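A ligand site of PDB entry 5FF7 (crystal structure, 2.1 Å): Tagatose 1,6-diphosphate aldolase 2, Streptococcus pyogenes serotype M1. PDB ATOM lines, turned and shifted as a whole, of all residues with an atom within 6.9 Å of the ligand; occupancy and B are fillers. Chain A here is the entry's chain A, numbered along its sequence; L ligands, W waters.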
ATOM      1  N   ALA A  26      -5.555 -19.138 -22.614  1.00  0.00           N
ATOM      2  CA  ALA A  26      -5.878 -20.534 -22.361  1.00  0.00           C
ATOM      3  C   ALA A  26      -4.641 -21.242 -21.822  1.00  0.00           C
ATOM      4  O   ALA A  26      -3.602 -21.266 -22.481  1.00  0.00           O
ATOM      5  CB  ALA A  26      -6.363 -21.233 -23.630  1.00  0.00           C
ATOM      6  N   PHE A  27      -4.758 -21.809 -20.620  1.00  0.00           N
ATOM      7  CA  PHE A  27      -3.661 -22.563 -20.036  1.00  0.00           C
ATOM      8  C   PHE A  27      -4.205 -23.675 -19.150  1.00  0.00           C
ATOM      9  O   PHE A  27      -3.802 -23.846 -18.005  1.00  0.00           O
ATOM     10  CB  PHE A  27      -2.725 -21.631 -19.255  1.00  0.00           C
ATOM     11  CG  PHE A  27      -1.333 -22.190 -19.040  1.00  0.00           C
ATOM     12  CD1 PHE A  27      -1.013 -23.489 -19.417  1.00  0.00           C
ATOM     13  CD2 PHE A  27      -0.348 -21.415 -18.462  1.00  0.00           C
ATOM     14  CE1 PHE A  27       0.253 -23.997 -19.224  1.00  0.00           C
ATOM     15  CE2 PHE A  27       0.923 -21.915 -18.263  1.00  0.00           C
ATOM     16  CZ  PHE A  27       1.225 -23.206 -18.638  1.00  0.00           C
ATOM     17  N   ASP A  28      -5.141 -24.455 -19.687  1.00  0.00           N
ATOM     18  CA  ASP A  28      -5.634 -25.647 -19.014  1.00  0.00           C
ATOM     19  C   ASP A  28      -4.959 -26.913 -19.519  1.00  0.00           C
ATOM     20  O   ASP A  28      -5.368 -28.020 -19.138  1.00  0.00           O
ATOM     21  CB  ASP A  28      -7.156 -25.764 -19.186  1.00  0.00           C
ATOM     22  CG  ASP A  28      -7.561 -25.962 -20.632  1.00  0.00           C
ATOM     23  OD1 ASP A  28      -6.732 -25.693 -21.531  1.00  0.00           O
ATOM     24  OD2 ASP A  28      -8.715 -26.363 -20.871  1.00  0.00           O
ATOM     25  N   GLN A  29      -3.929 -26.783 -20.356  1.00  0.00           N
ATOM     26  CA  GLN A  29      -3.209 -27.939 -20.841  1.00  0.00           C
ATOM     27  C   GLN A  29      -2.556 -28.686 -19.685  1.00  0.00           C
ATOM     28  O   GLN A  29      -1.946 -28.068 -18.798  1.00  0.00           O
ATOM     29  CB  GLN A  29      -2.149 -27.524 -21.861  1.00  0.00           C
ATOM     30  CG  GLN A  29      -2.705 -27.093 -23.210  1.00  0.00           C
ATOM     31  CD  GLN A  29      -3.268 -25.684 -23.209  1.00  0.00           C
ATOM     32  OE1 GLN A  29      -3.285 -25.019 -22.174  1.00  0.00           O
ATOM     33  NE2 GLN A  29      -3.709 -25.220 -24.361  1.00  0.00           N
ATOM     34  N   LEU A  69      -8.399 -19.257 -18.899  1.00  0.00           N
ATOM     35  CA  LEU A  69      -8.916 -20.605 -18.740  1.00  0.00           C
ATOM     36  C   LEU A  69      -7.844 -21.463 -18.072  1.00  0.00           C
ATOM     37  O   LEU A  69      -6.706 -21.510 -18.538  1.00  0.00           O
ATOM     38  CB  LEU A  69      -9.299 -21.203 -20.096  1.00  0.00           C
ATOM     39  CG  LEU A  69      -9.478 -22.726 -20.180  1.00  0.00           C
ATOM     40  CD1 LEU A  69     -10.617 -23.190 -19.289  1.00  0.00           C
ATOM     41  CD2 LEU A  69      -9.693 -23.157 -21.617  1.00  0.00           C
ATOM     42  N   ALA A  91     -11.649 -25.771 -16.717  1.00  0.00           N
ATOM     43  CA  ALA A  91     -11.882 -26.959 -17.518  1.00  0.00           C
ATOM     44  C   ALA A  91     -12.562 -28.031 -16.688  1.00  0.00           C
ATOM     45  O   ALA A  91     -12.304 -28.172 -15.486  1.00  0.00           O
ATOM     46  CB  ALA A  91     -10.561 -27.475 -18.082  1.00  0.00           C
ATOM     47  N   GLU A  93     -13.213 -31.402 -18.260  1.00  0.00           N
ATOM     48  CA  GLU A  93     -12.951 -32.715 -18.812  1.00  0.00           C
ATOM     49  C   GLU A  93     -11.606 -33.248 -18.334  1.00  0.00           C
ATOM     50  O   GLU A  93     -10.709 -32.500 -17.944  1.00  0.00           O
ATOM     51  CB  GLU A  93     -12.979 -32.684 -20.351  1.00  0.00           C
ATOM     52  CG  GLU A  93     -11.719 -32.131 -21.032  1.00  0.00           C
ATOM     53  CD  GLU A  93     -11.601 -30.624 -20.932  1.00  0.00           C
ATOM     54  OE1 GLU A  93     -12.556 -29.960 -20.491  1.00  0.00           O
ATOM     55  OE2 GLU A  93     -10.526 -30.092 -21.306  1.00  0.00           O
ATOM     56  N   LYS A 126     -15.823 -24.935 -19.021  1.00  0.00           N
ATOM     57  CA  LYS A 126     -15.269 -25.289 -20.311  1.00  0.00           C
ATOM     58  C   LYS A 126     -15.156 -26.805 -20.417  1.00  0.00           C
ATOM     59  O   LYS A 126     -14.728 -27.465 -19.455  1.00  0.00           O
ATOM     60  CB  LYS A 126     -13.906 -24.629 -20.532  1.00  0.00           C
ATOM     61  CG  LYS A 126     -13.211 -25.040 -21.824  1.00  0.00           C
ATOM     62  CD  LYS A 126     -12.201 -26.141 -21.577  1.00  0.00           C
ATOM     63  CE  LYS A 126     -11.542 -26.604 -22.861  1.00  0.00           C
ATOM     64  NZ  LYS A 126     -10.569 -27.694 -22.601  1.00  0.00           N
ATOM     65  N   LEU A 128     -14.029 -29.977 -23.338  1.00  0.00           N
ATOM     66  CA  LEU A 128     -13.463 -30.353 -24.627  1.00  0.00           C
ATOM     67  C   LEU A 128     -14.079 -31.650 -25.103  1.00  0.00           C
ATOM     68  O   LEU A 128     -14.098 -32.652 -24.363  1.00  0.00           O
ATOM     69  CB  LEU A 128     -11.948 -30.480 -24.532  1.00  0.00           C
ATOM     70  CG  LEU A 128     -11.248 -31.141 -25.734  1.00  0.00           C
ATOM     71  CD1 LEU A 128     -11.580 -30.426 -27.030  1.00  0.00           C
ATOM     72  CD2 LEU A 128      -9.747 -31.176 -25.508  1.00  0.00           C
ATOM     73  N   GLU A 164     -15.617 -26.726 -26.283  1.00  0.00           N
ATOM     74  CA  GLU A 164     -14.544 -26.807 -27.263  1.00  0.00           C
ATOM     75  C   GLU A 164     -14.709 -28.083 -28.076  1.00  0.00           C
ATOM     76  O   GLU A 164     -14.867 -29.174 -27.512  1.00  0.00           O
ATOM     77  CB  GLU A 164     -13.174 -26.798 -26.584  1.00  0.00           C
ATOM     78  CG  GLU A 164     -11.999 -26.882 -27.550  1.00  0.00           C
ATOM     79  CD  GLU A 164     -10.652 -26.930 -26.851  1.00  0.00           C
ATOM     80  OE1 GLU A 164     -10.627 -26.917 -25.609  1.00  0.00           O
ATOM     81  OE2 GLU A 164      -9.623 -26.983 -27.555  1.00  0.00           O
ATOM     82  N   LEU A 166     -12.832 -30.319 -30.906  1.00  0.00           N
ATOM     83  CA  LEU A 166     -11.688 -30.679 -31.720  1.00  0.00           C
ATOM     84  C   LEU A 166     -12.083 -31.842 -32.627  1.00  0.00           C
ATOM     85  O   LEU A 166     -12.563 -32.877 -32.138  1.00  0.00           O
ATOM     86  CB  LEU A 166     -10.476 -31.057 -30.860  1.00  0.00           C
ATOM     87  CG  LEU A 166      -9.871 -29.910 -30.063  1.00  0.00           C
ATOM     88  CD1 LEU A 166      -8.738 -30.412 -29.176  1.00  0.00           C
ATOM     89  CD2 LEU A 166      -9.360 -28.807 -30.984  1.00  0.00           C
ATOM     90  N   LYS A 206     -15.920 -22.976 -28.819  1.00  0.00           N
ATOM     91  CA  LYS A 206     -14.495 -22.802 -29.072  1.00  0.00           C
ATOM     92  C   LYS A 206     -14.098 -23.805 -30.147  1.00  0.00           C
ATOM     93  O   LYS A 206     -14.181 -25.022 -29.920  1.00  0.00           O
ATOM     94  CB  LYS A 206     -13.685 -23.008 -27.801  1.00  0.00           C
ATOM     95  CG  LYS A 206     -12.177 -22.985 -27.994  1.00  0.00           C
ATOM     96  CD  LYS A 206     -11.443 -23.286 -26.702  1.00  0.00           C
ATOM     97  CE  LYS A 206      -9.949 -23.463 -26.931  1.00  0.00           C
ATOM     98  NZ  LYS A 206      -9.213 -23.834 -25.696  1.00  0.00           N
ATOM     99  N   TYR A 248     -12.027 -18.734 -31.675  1.00  0.00           N
ATOM    100  CA  TYR A 248     -11.024 -19.587 -32.291  1.00  0.00           C
ATOM    101  C   TYR A 248      -9.951 -19.973 -31.290  1.00  0.00           C
ATOM    102  O   TYR A 248      -9.520 -19.170 -30.468  1.00  0.00           O
ATOM    103  CB  TYR A 248     -10.376 -18.877 -33.484  1.00  0.00           C
ATOM    104  CG  TYR A 248     -11.277 -18.718 -34.692  1.00  0.00           C
ATOM    105  CD1 TYR A 248     -12.059 -19.763 -35.149  1.00  0.00           C
ATOM    106  CD2 TYR A 248     -11.323 -17.519 -35.385  1.00  0.00           C
ATOM    107  CE1 TYR A 248     -12.874 -19.620 -36.256  1.00  0.00           C
ATOM    108  CE2 TYR A 248     -12.119 -17.360 -36.491  1.00  0.00           C
ATOM    109  CZ  TYR A 248     -12.899 -18.409 -36.927  1.00  0.00           C
ATOM    110  OH  TYR A 248     -13.701 -18.263 -38.030  1.00  0.00           O
ATOM    111  N   LEU A 249      -9.517 -21.225 -31.378  1.00  0.00           N
ATOM    112  CA  LEU A 249      -8.339 -21.712 -30.679  1.00  0.00           C
ATOM    113  C   LEU A 249      -7.144 -21.648 -31.617  1.00  0.00           C
ATOM    114  O   LEU A 249      -7.287 -21.653 -32.848  1.00  0.00           O
ATOM    115  CB  LEU A 249      -8.548 -23.142 -30.176  1.00  0.00           C
ATOM    116  CG  LEU A 249      -8.908 -24.182 -31.239  1.00  0.00           C
ATOM    117  CD1 LEU A 249      -7.674 -24.978 -31.637  1.00  0.00           C
ATOM    118  CD2 LEU A 249     -10.014 -25.099 -30.735  1.00  0.00           C
ATOM    119  N   SER A 250      -5.943 -21.586 -31.038  1.00  0.00           N
ATOM    120  CA  SER A 250      -4.742 -21.391 -31.842  1.00  0.00           C
ATOM    121  C   SER A 250      -4.222 -22.694 -32.432  1.00  0.00           C
ATOM    122  O   SER A 250      -3.558 -22.671 -33.481  1.00  0.00           O
ATOM    123  CB  SER A 250      -3.644 -20.720 -31.013  1.00  0.00           C
ATOM    124  OG  SER A 250      -3.064 -21.632 -30.096  1.00  0.00           O
ATOM    125  N   ALA A 251      -4.500 -23.824 -31.792  1.00  0.00           N
ATOM    126  CA  ALA A 251      -3.999 -25.128 -32.217  1.00  0.00           C
ATOM    127  C   ALA A 251      -2.479 -25.191 -32.211  1.00  0.00           C
ATOM    128  O   ALA A 251      -1.882 -26.061 -32.866  1.00  0.00           O
ATOM    129  CB  ALA A 251      -4.534 -25.494 -33.613  1.00  0.00           C
ATOM    130  N   GLY A 252      -1.829 -24.301 -31.478  1.00  0.00           N
ATOM    131  CA  GLY A 252      -0.383 -24.354 -31.333  1.00  0.00           C
ATOM    132  C   GLY A 252       0.396 -23.880 -32.539  1.00  0.00           C
ATOM    133  O   GLY A 252       1.592 -24.185 -32.634  1.00  0.00           O
ATOM    134  N   VAL A 253      -0.217 -23.151 -33.461  1.00  0.00           N
ATOM    135  CA  VAL A 253       0.513 -22.554 -34.570  1.00  0.00           C
ATOM    136  C   VAL A 253       1.307 -21.375 -34.024  1.00  0.00           C
ATOM    137  O   VAL A 253       1.099 -20.955 -32.878  1.00  0.00           O
ATOM    138  CB  VAL A 253      -0.423 -22.118 -35.711  1.00  0.00           C
ATOM    139  CG1 VAL A 253      -1.211 -23.312 -36.242  1.00  0.00           C
ATOM    140  CG2 VAL A 253      -1.359 -21.001 -35.260  1.00  0.00           C
ATOM    141  N   PHE A 258      -1.264 -17.373 -36.548  1.00  0.00           N
ATOM    142  CA  PHE A 258      -2.585 -17.232 -35.965  1.00  0.00           C
ATOM    143  C   PHE A 258      -3.140 -15.824 -36.193  1.00  0.00           C
ATOM    144  O   PHE A 258      -4.300 -15.665 -36.561  1.00  0.00           O
ATOM    145  CB  PHE A 258      -2.530 -17.564 -34.474  1.00  0.00           C
ATOM    146  CG  PHE A 258      -3.878 -17.641 -33.821  1.00  0.00           C
ATOM    147  CD1 PHE A 258      -4.852 -18.494 -34.304  1.00  0.00           C
ATOM    148  CD2 PHE A 258      -4.175 -16.858 -32.717  1.00  0.00           C
ATOM    149  CE1 PHE A 258      -6.086 -18.572 -33.705  1.00  0.00           C
ATOM    150  CE2 PHE A 258      -5.415 -16.929 -32.103  1.00  0.00           C
ATOM    151  CZ  PHE A 258      -6.373 -17.788 -32.611  1.00  0.00           C
ATOM    152  N   LEU A 276      -9.670 -18.092 -27.653  1.00  0.00           N
ATOM    153  CA  LEU A 276      -9.131 -18.680 -26.434  1.00  0.00           C
ATOM    154  C   LEU A 276      -7.756 -19.183 -26.836  1.00  0.00           C
ATOM    155  O   LEU A 276      -7.587 -20.348 -27.233  1.00  0.00           O
ATOM    156  CB  LEU A 276     -10.027 -19.786 -25.865  1.00  0.00           C
ATOM    157  CG  LEU A 276     -10.689 -19.465 -24.518  1.00  0.00           C
ATOM    158  CD1 LEU A 276     -11.712 -20.537 -24.151  1.00  0.00           C
ATOM    159  CD2 LEU A 276      -9.646 -19.318 -23.425  1.00  0.00           C
ATOM    160  N   CYS A 277      -6.773 -18.293 -26.761  1.00  0.00           N
ATOM    161  CA  CYS A 277      -5.450 -18.526 -27.332  1.00  0.00           C
ATOM    162  C   CYS A 277      -4.506 -18.981 -26.227  1.00  0.00           C
ATOM    163  O   CYS A 277      -4.348 -18.296 -25.212  1.00  0.00           O
ATOM    164  CB  CYS A 277      -4.928 -17.252 -28.008  1.00  0.00           C
ATOM    165  SG  CYS A 277      -3.361 -17.469 -28.854  1.00  0.00           S
ATOM    166  N   GLY A 278      -3.872 -20.133 -26.423  1.00  0.00           N
ATOM    167  CA  GLY A 278      -2.945 -20.668 -25.458  1.00  0.00           C
ATOM    168  C   GLY A 278      -1.529 -20.755 -25.966  1.00  0.00           C
ATOM    169  O   GLY A 278      -0.731 -19.814 -25.791  1.00  0.00           O
ATOM    170  N   ARG A 279      -1.199 -21.874 -26.610  1.00  0.00           N
ATOM    171  CA  ARG A 279       0.193 -22.157 -26.949  1.00  0.00           C
ATOM    172  C   ARG A 279       0.810 -21.064 -27.812  1.00  0.00           C
ATOM    173  O   ARG A 279       1.966 -20.672 -27.602  1.00  0.00           O
ATOM    174  CB  ARG A 279       0.290 -23.509 -27.649  1.00  0.00           C
ATOM    175  CG  ARG A 279       0.113 -24.694 -26.704  1.00  0.00           C
ATOM    176  CD  ARG A 279      -0.240 -25.965 -27.447  1.00  0.00           C
ATOM    177  NE  ARG A 279      -1.586 -25.888 -28.019  1.00  0.00           N
ATOM    178  CZ  ARG A 279      -2.146 -26.849 -28.748  1.00  0.00           C
ATOM    179  NH1 ARG A 279      -1.473 -27.970 -29.000  1.00  0.00           N
ATOM    180  NH2 ARG A 279      -3.371 -26.695 -29.225  1.00  0.00           N
ATOM    181  N   ALA A 280       0.058 -20.537 -28.779  1.00  0.00           N
ATOM    182  CA  ALA A 280       0.595 -19.495 -29.640  1.00  0.00           C
ATOM    183  C   ALA A 280       1.114 -18.294 -28.845  1.00  0.00           C
ATOM    184  O   ALA A 280       1.948 -17.542 -29.355  1.00  0.00           O
ATOM    185  CB  ALA A 280      -0.473 -19.031 -30.638  1.00  0.00           C
ATOM    186  N   THR A 281       0.652 -18.127 -27.603  1.00  0.00           N
ATOM    187  CA  THR A 281       1.098 -17.019 -26.773  1.00  0.00           C
ATOM    188  C   THR A 281       2.274 -17.389 -25.877  1.00  0.00           C
ATOM    189  O   THR A 281       3.299 -16.686 -25.882  1.00  0.00           O
ATOM    190  CB  THR A 281      -0.075 -16.525 -25.911  1.00  0.00           C
ATOM    191  OG1 THR A 281      -1.071 -15.940 -26.758  1.00  0.00           O
ATOM    192  CG2 THR A 281       0.385 -15.475 -24.887  1.00  0.00           C
ATOM    193  N   TRP A 282       2.171 -18.475 -25.121  1.00  0.00           N
ATOM    194  CA  TRP A 282       3.130 -18.790 -24.067  1.00  0.00           C
ATOM    195  C   TRP A 282       3.999 -20.006 -24.351  1.00  0.00           C
ATOM    196  O   TRP A 282       4.791 -20.393 -23.492  1.00  0.00           O
ATOM    197  CB  TRP A 282       2.394 -19.009 -22.736  1.00  0.00           C
ATOM    198  CG  TRP A 282       1.254 -19.994 -22.800  1.00  0.00           C
ATOM    199  CD1 TRP A 282      -0.077 -19.687 -22.857  1.00  0.00           C
ATOM    200  CD2 TRP A 282       1.344 -21.424 -22.817  1.00  0.00           C
ATOM    201  NE1 TRP A 282      -0.823 -20.837 -22.907  1.00  0.00           N
ATOM    202  CE2 TRP A 282       0.024 -21.923 -22.882  1.00  0.00           C
ATOM    203  CE3 TRP A 282       2.405 -22.327 -22.782  1.00  0.00           C
ATOM    204  CZ2 TRP A 282      -0.258 -23.279 -22.921  1.00  0.00           C
ATOM    205  CZ3 TRP A 282       2.123 -23.682 -22.821  1.00  0.00           C
ATOM    206  CH2 TRP A 282       0.801 -24.141 -22.884  1.00  0.00           C
HETATM  207  O1  LIG L   1      -8.271 -25.421 -23.765  1.00  0.00           O
HETATM  208  C1  LIG L   1      -7.290 -24.839 -24.592  1.00  0.00           C
HETATM  209  C2  LIG L   1      -7.948 -24.203 -25.798  1.00  0.00           C
HETATM  210  C3  LIG L   1      -6.954 -23.322 -26.536  1.00  0.00           C
HETATM  211  O2  LIG L   1      -5.726 -23.994 -26.649  1.00  0.00           O
HETATM  212  O3  LIG L   1      -4.963 -24.383 -29.061  1.00  0.00           O
HETATM  213  O4  LIG L   1      -3.313 -23.836 -27.491  1.00  0.00           O
HETATM  214  O5  LIG L   1      -4.797 -22.198 -28.257  1.00  0.00           O
HETATM  215  P1  LIG L   1      -4.740 -23.613 -27.823  1.00  0.00           P
HETATM  216  O   HOH W   1      -6.658 -26.707 -28.390  1.00  0.00           O
HETATM  217  O   HOH W   2      -6.476 -27.901 -22.923  1.00  0.00           O
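Water W1 lies within hydrogen-bond range of an oxygen (O3) of the ligand (3.0 Å), the side-chain carboxylate (OE2) of Glu 164 (3.1 Å) and the guanidinium group (NH2) of Arg 279 (3.4 Å). Water W2 lies within hydrogen-bond range of OD1 of Asp 28 (2.6 Å) and O1 of the ligand (3.2 Å).
The side-chain amino group of Lys 206 is covalently linked to a carbon (C2) of the ligand (1.3 Å). The backbone NH (N) of Ser 250 sits at hydrogen-bond distance from an oxygen (O5) of the ligand (3.1 Å). O5 of the ligand lies within hydrogen-bond range of OG of Ser 250 (2.6 Å). O1 of the ligand sits at hydrogen-bond distance from OD1 of Asp 28. N of Arg 279 is in hydrogen-bond range of O4 of the ligand, 3.0 Å away. NE of Arg 279 is in salt-bridge range of O4 of the ligand, 2.7 Å away. An oxygen (O3) of the ligand sits at hydrogen-bond distance from the backbone NH (N) of Ala 251, at 2.8 Å. N of Gly 278 lies within hydrogen-bond range of O5 of the ligand, at 2.9 Å. The side-chain amide nitrogen (NE2) of Gln 29 lies within hydrogen-bond range of an oxygen (O2) of the ligand (3.3 Å). O1 of the ligand lies within hydrogen-bond range of OE1 of Glu 164, at 3.3 Å. NZ of Lys 126 sits at hydrogen-bond distance from O1 of the ligand, at 3.4 Å.
Merely in contact with the ligand: Ala 26 (3.6 Å), Leu 69 (3.4 Å), Leu 249 (3.8 Å), Gly 252 (3.96 Å), Leu 276 (3.1 Å) and Cys 277 (3.8 Å). Hydrophobic or aromatic side chains within 4 Å of the ligand: Ala 26, Leu 69 and Leu 249. Within 4 Å of the ligand: Ala 26, Asp 28, Gln 29, Leu 69, Lys 126, Glu 164, Lys 206, Leu 249, Ser 250, Ala 251, Gly 252, Leu 276, Cys 277, Gly 278 and Arg 279. The nearest printed residue that does not touch the ligand is Ala 280 (4.9 Å).
The side-chain hydroxyl (OG) of Ser 250 lies close to the backbone NH (N) of Gly 252 (3.2 Å). The side-chain amino group (NZ) of Lys 126 is in salt-bridge range of the side-chain carboxylate (OD2) of Asp 28 (2.9 Å). The backbone carbonyl oxygen (O) of Gly 278 lies close to the indole nitrogen (NE1) of Trp 282. The side-chain amino group (NZ) of Lys 126 lies within salt-bridge range of the side-chain carboxylate (OE1) of Glu 164 (3.1 Å). The side-chain amino group of Lys 126 lies within salt-bridge range of the side-chain carboxylate of Glu 93. The backbone NH (N) of Ala 26 lies within hydrogen-bond range of the backbone carbonyl oxygen (O) of Cys 277, 3.0 Å away. The indole nitrogen (NE1) of Trp 282 lies within hydrogen-bond range of the backbone carbonyl oxygen (O) of Ala 26. The side-chain sulfur (SG) of Cys 277 is in hydrogen-bond range of the side-chain hydroxyl (OG1) of Thr 281, at 3.5 Å.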
